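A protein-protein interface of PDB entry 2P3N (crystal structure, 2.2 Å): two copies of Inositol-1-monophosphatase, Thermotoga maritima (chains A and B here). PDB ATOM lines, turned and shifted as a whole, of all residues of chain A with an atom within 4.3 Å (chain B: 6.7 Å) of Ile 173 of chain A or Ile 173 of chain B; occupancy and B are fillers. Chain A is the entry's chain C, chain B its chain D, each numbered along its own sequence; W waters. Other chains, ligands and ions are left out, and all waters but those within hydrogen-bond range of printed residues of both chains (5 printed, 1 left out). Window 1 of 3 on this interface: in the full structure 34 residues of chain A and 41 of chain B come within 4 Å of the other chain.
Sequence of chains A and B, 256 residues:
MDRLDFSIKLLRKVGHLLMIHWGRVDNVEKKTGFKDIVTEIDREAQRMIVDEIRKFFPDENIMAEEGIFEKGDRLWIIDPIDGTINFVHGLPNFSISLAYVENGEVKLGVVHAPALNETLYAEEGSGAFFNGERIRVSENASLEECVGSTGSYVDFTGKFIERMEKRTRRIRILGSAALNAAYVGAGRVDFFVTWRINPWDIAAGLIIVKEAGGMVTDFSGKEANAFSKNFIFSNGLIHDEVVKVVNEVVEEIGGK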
ATOM      1  N   THR A 150     -13.984  -0.428 -10.860  1.00  0.00           N
ATOM      2  CA  THR A 150     -14.759  -1.142  -9.856  1.00  0.00           C
ATOM      3  C   THR A 150     -15.907  -0.263  -9.430  1.00  0.00           C
ATOM      4  O   THR A 150     -16.105   0.826  -9.974  1.00  0.00           O
ATOM      5  CB  THR A 150     -13.950  -1.480  -8.584  1.00  0.00           C
ATOM      6  OG1 THR A 150     -13.161  -0.351  -8.198  1.00  0.00           O
ATOM      7  CG2 THR A 150     -13.064  -2.667  -8.819  1.00  0.00           C
ATOM      8  N   SER A 152     -18.327   1.256  -5.926  1.00  0.00           N
ATOM      9  CA  SER A 152     -18.031   1.953  -4.683  1.00  0.00           C
ATOM     10  C   SER A 152     -18.382   1.077  -3.482  1.00  0.00           C
ATOM     11  O   SER A 152     -19.555   0.912  -3.140  1.00  0.00           O
ATOM     12  CB  SER A 152     -18.798   3.275  -4.641  1.00  0.00           C
ATOM     13  OG  SER A 152     -18.486   4.058  -5.785  1.00  0.00           O
ATOM     14  N   ILE A 161      -7.882   0.393  -5.329  1.00  0.00           N
ATOM     15  CA  ILE A 161      -7.201   1.479  -6.013  1.00  0.00           C
ATOM     16  C   ILE A 161      -5.721   1.589  -5.641  1.00  0.00           C
ATOM     17  O   ILE A 161      -4.891   1.923  -6.481  1.00  0.00           O
ATOM     18  CB  ILE A 161      -7.887   2.828  -5.733  1.00  0.00           C
ATOM     19  CG1 ILE A 161      -9.304   2.819  -6.307  1.00  0.00           C
ATOM     20  CG2 ILE A 161      -7.072   3.955  -6.336  1.00  0.00           C
ATOM     21  CD1 ILE A 161     -10.020   4.156  -6.201  1.00  0.00           C
ATOM     22  N   ILE A 171      -7.642   3.620 -13.031  1.00  0.00           N
ATOM     23  CA  ILE A 171      -8.814   2.871 -12.579  1.00  0.00           C
ATOM     24  C   ILE A 171      -9.940   3.897 -12.600  1.00  0.00           C
ATOM     25  O   ILE A 171      -9.739   5.040 -12.181  1.00  0.00           O
ATOM     26  CB  ILE A 171      -8.677   2.338 -11.123  1.00  0.00           C
ATOM     27  CG1 ILE A 171      -7.468   1.407 -10.986  1.00  0.00           C
ATOM     28  CG2 ILE A 171      -9.938   1.574 -10.739  1.00  0.00           C
ATOM     29  CD1 ILE A 171      -7.603   0.111 -11.744  1.00  0.00           C
ATOM     30  N   ARG A 172     -11.111   3.480 -13.082  1.00  0.00           N
ATOM     31  CA  ARG A 172     -12.283   4.352 -13.203  1.00  0.00           C
ATOM     32  C   ARG A 172     -13.463   3.923 -12.332  1.00  0.00           C
ATOM     33  O   ARG A 172     -13.712   2.734 -12.124  1.00  0.00           O
ATOM     34  CB  ARG A 172     -12.745   4.404 -14.668  1.00  0.00           C
ATOM     35  CG  ARG A 172     -11.759   5.056 -15.627  1.00  0.00           C
ATOM     36  CD  ARG A 172     -11.942   6.579 -15.689  1.00  0.00           C
ATOM     37  NE  ARG A 172     -10.889   7.247 -16.455  1.00  0.00           N
ATOM     38  CZ  ARG A 172      -9.780   7.758 -15.924  1.00  0.00           C
ATOM     39  NH1 ARG A 172      -9.572   7.684 -14.616  1.00  0.00           N
ATOM     40  NH2 ARG A 172      -8.882   8.354 -16.696  1.00  0.00           N
ATOM     41  N   ILE A 173     -14.190   4.908 -11.827  1.00  0.00           N
ATOM     42  CA  ILE A 173     -15.357   4.645 -11.004  1.00  0.00           C
ATOM     43  C   ILE A 173     -16.428   5.513 -11.633  1.00  0.00           C
ATOM     44  O   ILE A 173     -16.566   6.688 -11.299  1.00  0.00           O
ATOM     45  CB  ILE A 173     -15.115   5.062  -9.550  1.00  0.00           C
ATOM     46  CG1 ILE A 173     -13.782   4.483  -9.079  1.00  0.00           C
ATOM     47  CG2 ILE A 173     -16.263   4.559  -8.663  1.00  0.00           C
ATOM     48  CD1 ILE A 173     -13.296   5.039  -7.780  1.00  0.00           C
ATOM     49  N   LEU A 174     -17.175   4.913 -12.556  1.00  0.00           N
ATOM     50  CA  LEU A 174     -18.202   5.616 -13.294  1.00  0.00           C
ATOM     51  C   LEU A 174     -19.596   5.595 -12.692  1.00  0.00           C
ATOM     52  O   LEU A 174     -20.352   6.555 -12.878  1.00  0.00           O
ATOM     53  CB  LEU A 174     -18.236   5.098 -14.728  1.00  0.00           C
ATOM     54  CG  LEU A 174     -16.899   5.356 -15.419  1.00  0.00           C
ATOM     55  CD1 LEU A 174     -17.069   5.161 -16.910  1.00  0.00           C
ATOM     56  CD2 LEU A 174     -16.412   6.784 -15.100  1.00  0.00           C
ATOM     57  N   GLY A 175     -19.970   4.512 -12.013  1.00  0.00           N
ATOM     58  CA  GLY A 175     -21.277   4.516 -11.374  1.00  0.00           C
ATOM     59  C   GLY A 175     -22.402   3.577 -11.758  1.00  0.00           C
ATOM     60  O   GLY A 175     -23.404   3.528 -11.033  1.00  0.00           O
ATOM     61  N   ASN B  93     -15.871  10.081 -21.507  1.00  0.00           N
ATOM     62  CA  ASN B  93     -15.432  11.183 -20.647  1.00  0.00           C
ATOM     63  C   ASN B  93     -14.095  11.805 -21.019  1.00  0.00           C
ATOM     64  O   ASN B  93     -13.066  11.526 -20.408  1.00  0.00           O
ATOM     65  CB  ASN B  93     -15.368  10.766 -19.169  1.00  0.00           C
ATOM     66  CG  ASN B  93     -16.731  10.396 -18.593  1.00  0.00           C
ATOM     67  OD1 ASN B  93     -17.770  10.815 -19.091  1.00  0.00           O
ATOM     68  ND2 ASN B  93     -16.721   9.616 -17.521  1.00  0.00           N
ATOM     69  N   GLY B 148     -18.687  13.235  -4.298  1.00  0.00           N
ATOM     70  CA  GLY B 148     -17.429  13.911  -4.579  1.00  0.00           C
ATOM     71  C   GLY B 148     -16.679  13.217  -5.694  1.00  0.00           C
ATOM     72  O   GLY B 148     -17.174  12.239  -6.249  1.00  0.00           O
ATOM     73  N   SER B 149     -15.490  13.699  -6.031  1.00  0.00           N
ATOM     74  CA  SER B 149     -14.730  13.080  -7.106  1.00  0.00           C
ATOM     75  C   SER B 149     -13.262  13.431  -7.037  1.00  0.00           C
ATOM     76  O   SER B 149     -12.894  14.447  -6.450  1.00  0.00           O
ATOM     77  CB  SER B 149     -15.307  13.503  -8.466  1.00  0.00           C
ATOM     78  OG  SER B 149     -15.490  14.906  -8.546  1.00  0.00           O
ATOM     79  N   THR B 150     -12.427  12.592  -7.644  1.00  0.00           N
ATOM     80  CA  THR B 150     -10.981  12.809  -7.637  1.00  0.00           C
ATOM     81  C   THR B 150     -10.357  12.433  -8.959  1.00  0.00           C
ATOM     82  O   THR B 150     -11.019  11.866  -9.827  1.00  0.00           O
ATOM     83  CB  THR B 150     -10.281  11.920  -6.609  1.00  0.00           C
ATOM     84  OG1 THR B 150     -11.204  11.558  -5.577  1.00  0.00           O
ATOM     85  CG2 THR B 150      -9.080  12.637  -6.023  1.00  0.00           C
ATOM     86  N   GLY B 151      -9.066  12.736  -9.083  1.00  0.00           N
ATOM     87  CA  GLY B 151      -8.308  12.376 -10.270  1.00  0.00           C
ATOM     88  C   GLY B 151      -7.564  11.123  -9.849  1.00  0.00           C
ATOM     89  O   GLY B 151      -7.574  10.815  -8.659  1.00  0.00           O
ATOM     90  N   SER B 152      -6.937  10.399 -10.774  1.00  0.00           N
ATOM     91  CA  SER B 152      -6.211   9.177 -10.412  1.00  0.00           C
ATOM     92  C   SER B 152      -4.756   9.441 -10.036  1.00  0.00           C
ATOM     93  O   SER B 152      -3.870   9.362 -10.882  1.00  0.00           O
ATOM     94  CB  SER B 152      -6.260   8.166 -11.558  1.00  0.00           C
ATOM     95  OG  SER B 152      -7.562   7.639 -11.721  1.00  0.00           O
ATOM     96  N   THR B 157      -5.382   9.496  -4.328  1.00  0.00           N
ATOM     97  CA  THR B 157      -6.619   8.754  -4.581  1.00  0.00           C
ATOM     98  C   THR B 157      -7.029   7.706  -3.546  1.00  0.00           C
ATOM     99  O   THR B 157      -7.981   7.926  -2.804  1.00  0.00           O
ATOM    100  CB  THR B 157      -6.588   8.062  -5.956  1.00  0.00           C
ATOM    101  OG1 THR B 157      -6.181   8.997  -6.958  1.00  0.00           O
ATOM    102  CG2 THR B 157      -7.971   7.540  -6.307  1.00  0.00           C
ATOM    103  N   ILE B 161     -10.222   8.085  -1.115  1.00  0.00           N
ATOM    104  CA  ILE B 161     -11.346   7.161  -1.251  1.00  0.00           C
ATOM    105  C   ILE B 161     -11.662   6.607   0.120  1.00  0.00           C
ATOM    106  O   ILE B 161     -12.818   6.525   0.514  1.00  0.00           O
ATOM    107  CB  ILE B 161     -11.001   5.938  -2.142  1.00  0.00           C
ATOM    108  CG1 ILE B 161     -10.517   6.384  -3.529  1.00  0.00           C
ATOM    109  CG2 ILE B 161     -12.214   5.019  -2.244  1.00  0.00           C
ATOM    110  CD1 ILE B 161     -11.555   7.084  -4.372  1.00  0.00           C
ATOM    111  N   ARG B 170     -20.942   8.499  -2.712  1.00  0.00           N
ATOM    112  CA  ARG B 170     -19.954   7.905  -3.609  1.00  0.00           C
ATOM    113  C   ARG B 170     -18.909   8.911  -4.047  1.00  0.00           C
ATOM    114  O   ARG B 170     -19.163  10.108  -4.046  1.00  0.00           O
ATOM    115  CB  ARG B 170     -20.648   7.326  -4.848  1.00  0.00           C
ATOM    116  CG  ARG B 170     -21.129   5.901  -4.646  1.00  0.00           C
ATOM    117  CD  ARG B 170     -22.241   5.539  -5.599  1.00  0.00           C
ATOM    118  NE  ARG B 170     -22.795   4.197  -5.379  1.00  0.00           N
ATOM    119  CZ  ARG B 170     -23.100   3.679  -4.192  1.00  0.00           C
ATOM    120  NH1 ARG B 170     -22.900   4.362  -3.081  1.00  0.00           N
ATOM    121  NH2 ARG B 170     -23.654   2.482  -4.125  1.00  0.00           N
ATOM    122  N   ILE B 171     -17.720   8.423  -4.390  1.00  0.00           N
ATOM    123  CA  ILE B 171     -16.646   9.277  -4.892  1.00  0.00           C
ATOM    124  C   ILE B 171     -16.413   8.758  -6.309  1.00  0.00           C
ATOM    125  O   ILE B 171     -16.243   7.555  -6.516  1.00  0.00           O
ATOM    126  CB  ILE B 171     -15.339   9.137  -4.071  1.00  0.00           C
ATOM    127  CG1 ILE B 171     -15.559   9.603  -2.628  1.00  0.00           C
ATOM    128  CG2 ILE B 171     -14.226   9.960  -4.726  1.00  0.00           C
ATOM    129  CD1 ILE B 171     -15.729  11.091  -2.473  1.00  0.00           C
ATOM    130  N   ARG B 172     -16.423   9.658  -7.283  1.00  0.00           N
ATOM    131  CA  ARG B 172     -16.252   9.270  -8.679  1.00  0.00           C
ATOM    132  C   ARG B 172     -14.891   9.623  -9.259  1.00  0.00           C
ATOM    133  O   ARG B 172     -14.287  10.629  -8.893  1.00  0.00           O
ATOM    134  CB  ARG B 172     -17.335   9.943  -9.528  1.00  0.00           C
ATOM    135  CG  ARG B 172     -18.746   9.479  -9.238  1.00  0.00           C
ATOM    136  CD  ARG B 172     -19.171   8.353 -10.168  1.00  0.00           C
ATOM    137  NE  ARG B 172     -20.431   7.732  -9.748  1.00  0.00           N
ATOM    138  CZ  ARG B 172     -20.531   6.700  -8.906  1.00  0.00           C
ATOM    139  NH1 ARG B 172     -19.439   6.150  -8.380  1.00  0.00           N
ATOM    140  NH2 ARG B 172     -21.727   6.211  -8.591  1.00  0.00           N
ATOM    141  N   ILE B 173     -14.410   8.773 -10.160  1.00  0.00           N
ATOM    142  CA  ILE B 173     -13.152   9.016 -10.861  1.00  0.00           C
ATOM    143  C   ILE B 173     -13.555   8.880 -12.320  1.00  0.00           C
ATOM    144  O   ILE B 173     -13.708   7.777 -12.834  1.00  0.00           O
ATOM    145  CB  ILE B 173     -12.077   7.991 -10.515  1.00  0.00           C
ATOM    146  CG1 ILE B 173     -11.773   8.068  -9.019  1.00  0.00           C
ATOM    147  CG2 ILE B 173     -10.817   8.270 -11.345  1.00  0.00           C
ATOM    148  CD1 ILE B 173     -10.906   6.954  -8.500  1.00  0.00           C
ATOM    149  N   LEU B 174     -13.736  10.026 -12.967  1.00  0.00           N
ATOM    150  CA  LEU B 174     -14.199  10.095 -14.339  1.00  0.00           C
ATOM    151  C   LEU B 174     -13.160  10.072 -15.445  1.00  0.00           C
ATOM    152  O   LEU B 174     -13.372   9.423 -16.478  1.00  0.00           O
ATOM    153  CB  LEU B 174     -15.078  11.333 -14.469  1.00  0.00           C
ATOM    154  CG  LEU B 174     -16.237  11.310 -13.464  1.00  0.00           C
ATOM    155  CD1 LEU B 174     -16.969  12.640 -13.529  1.00  0.00           C
ATOM    156  CD2 LEU B 174     -17.184  10.122 -13.757  1.00  0.00           C
ATOM    157  N   GLY B 175     -12.057  10.790 -15.252  1.00  0.00           N
ATOM    158  CA  GLY B 175     -11.018  10.808 -16.263  1.00  0.00           C
ATOM    159  C   GLY B 175     -10.855  12.079 -17.083  1.00  0.00           C
ATOM    160  O   GLY B 175     -10.101  12.085 -18.055  1.00  0.00           O
ATOM    161  N   SER B 176     -11.568  13.142 -16.725  1.00  0.00           N
ATOM    162  CA  SER B 176     -11.438  14.410 -17.438  1.00  0.00           C
ATOM    163  C   SER B 176     -11.602  15.580 -16.475  1.00  0.00           C
ATOM    164  O   SER B 176     -12.706  15.991 -16.166  1.00  0.00           O
ATOM    165  CB  SER B 176     -12.462  14.515 -18.565  1.00  0.00           C
ATOM    166  OG  SER B 176     -12.325  15.758 -19.233  1.00  0.00           O
ATOM    167  N   ASN B 180     -14.885  17.308 -15.124  1.00  0.00           N
ATOM    168  CA  ASN B 180     -15.201  17.023 -13.728  1.00  0.00           C
ATOM    169  C   ASN B 180     -15.402  18.321 -12.921  1.00  0.00           C
ATOM    170  O   ASN B 180     -16.285  18.398 -12.065  1.00  0.00           O
ATOM    171  CB  ASN B 180     -14.086  16.166 -13.116  1.00  0.00           C
ATOM    172  CG  ASN B 180     -14.609  15.148 -12.107  1.00  0.00           C
ATOM    173  OD1 ASN B 180     -14.048  14.051 -11.966  1.00  0.00           O
ATOM    174  ND2 ASN B 180     -15.683  15.509 -11.392  1.00  0.00           N
HETATM  175  O   HOH W   1      -8.287  10.286 -18.722  1.00  0.00           O
HETATM  176  O   HOH W   2     -22.283  -0.400  -4.211  1.00  0.00           O
HETATM  177  O   HOH W   3     -20.228   2.911  -8.006  1.00  0.00           O
HETATM  178  O   HOH W   4     -24.661   5.409  -8.946  1.00  0.00           O
HETATM  179  O   HOH W   5     -22.796   2.859  -8.440  1.00  0.00           O
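The backbone NH of Gly 148 of chain B sits at hydrogen-bond distance from the backbone carbonyl oxygen of Arg 170 of chain B, at 3.2 Å.
N of Thr 150 of chain B is in hydrogen-bond range of O of Arg 172 of chain B (3.0 Å).
O of Gly 148 of chain B is in hydrogen-bond range of N of Arg 172 of chain B (2.9 Å).
The backbone NH (N) of Thr 150 of chain A lies within hydrogen-bond range of the backbone carbonyl oxygen (O) of Arg 172 of chain A (3.4 Å).
O of Gly 151 of chain B lies within hydrogen-bond range of OG1 of Thr 157 of chain B (2.9 Å).
Water W1 bridges O of Gly 175 of chain B (2.6 Å) and NH2 of Arg 172 of chain A (2.9 Å).
Water W5 lies within hydrogen-bond range of the backbone carbonyl oxygen of Gly 175 of chain A (2.7 Å) and the guanidinium group of Arg 170 of chain B (3.3 Å).
Water W3 lies within hydrogen-bond range of OG of Ser 152 of chain A (3.0 Å) and NH1 of Arg 172 of chain B (3.4 Å).
Water W4 bridges NH2 of Arg 172 of chain B and O of Gly 175 of chain A.
Water W2 bridges NH2 of Arg 170 of chain B (3.2 Å) and O of Ser 152 of chain A (3.2 Å).
Among the printed residues, merely in contact across the chains: Ser 152 of chain A with Arg 170 of chain B (3.4 Å), Ile 161 of chain A with Thr 157 of chain B (3.7 Å), Ile 161 of chain A with Ile 161 of chain B (3.5 Å), Ile 161 of chain A with Ile 173 of chain B (3.7 Å), Ile 171 of chain A with Ile 173 of chain B (3.5 Å), Arg 172 of chain A with Ser 152 of chain B (3.5 Å), Arg 172 of chain A with Ile 173 of chain B (3.5 Å), Arg 172 of chain A with Gly 175 of chain B (3.3 Å), Ile 173 of chain A with Ile 171 of chain B (3.7 Å), Ile 173 of chain A with Arg 172 of chain B (3.3 Å), Leu 174 of chain A with Asn 93 of chain B (3.7 Å), Leu 174 of chain A with Ile 173 of chain B (3.7 Å), Leu 174 of chain A with Leu 174 of chain B (3.7 Å) and Gly 175 of chain A with Arg 172 of chain B (3.3 Å).
Of the 8 printed residues of chain A, 7 touch a printed residue of chain B.
Hydrophobic or aromatic side chains of chain A within 4 Å of the printed part of chain B: Ile 161, Ile 173 and Leu 174.
Among the printed residues, 19 pairs touch across the chains.
The side-chain hydroxyl (OG) of Ser 152 of chain A lies within hydrogen-bond range of the guanidinium group (NH1) of Arg 172 of chain B (3.5 Å).
NE of Arg 172 of chain A lies close to O of Leu 174 of chain B, at 3.3 Å.
The backbone carbonyl oxygen (O) of Leu 174 of chain A lies within hydrogen-bond range of the guanidinium group (NE) of Arg 172 of chain B (3.3 Å).
The side-chain hydroxyl (OG) of Ser 152 of chain B sits at hydrogen-bond distance from the backbone carbonyl oxygen (O) of Ile 171 of chain A (3.4 Å).
N of Ile 173 of chain A is in hydrogen-bond range of O of Ile 173 of chain B, at 3.1 Å.
Ile 161 of chain B touches its own counterpart, Ile 161 of chain A.
Arg 172 of chain A touches Ile 173 of chain B, and with the chains exchanged Ile 173 of chain A touches Arg 172 of chain B.
Arg 172 of chain A touches Leu 174 of chain B, and with the chains exchanged Leu 174 of chain A touches Arg 172 of chain B.
Ile 173 of chain A touches its own counterpart, Ile 173 of chain B.
Ile 173 of chain A touches just these residues of chain B: Ile 171, Arg 172 and Ile 173.
Ile 173 of chain B touches just these residues of chain A: Ile 161, Ile 171, Arg 172, Ile 173 and Leu 174.
Printed residues of chain B within 4 Å of Ile 161 of chain A: Thr 157 (3.7 Å), Ile 161 (3.5 Å) and Ile 173 (3.7 Å).
Printed residues of chain A within 4 Å of Arg 172 of chain B: Ser 152, Ile 173, Leu 174 and Gly 175.
Of the printed residues of chain A, Ser 152 of chain B touches Ile 171 (3.4 Å) and Arg 172 (3.5 Å).
Of the printed residues of chain A, Thr 157 of chain B touches Ile 161 (3.7 Å).
Asn 180 of chain B touches none of the printed residues of chain A.
The nearest printed residue of chain A that does not touch Ile 173 of chain B is Gly 175 of chain A (7.1 Å).
The nearest printed residue of chain A that does not touch Arg 172 of chain B is Thr 150 of chain A (6.5 Å).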
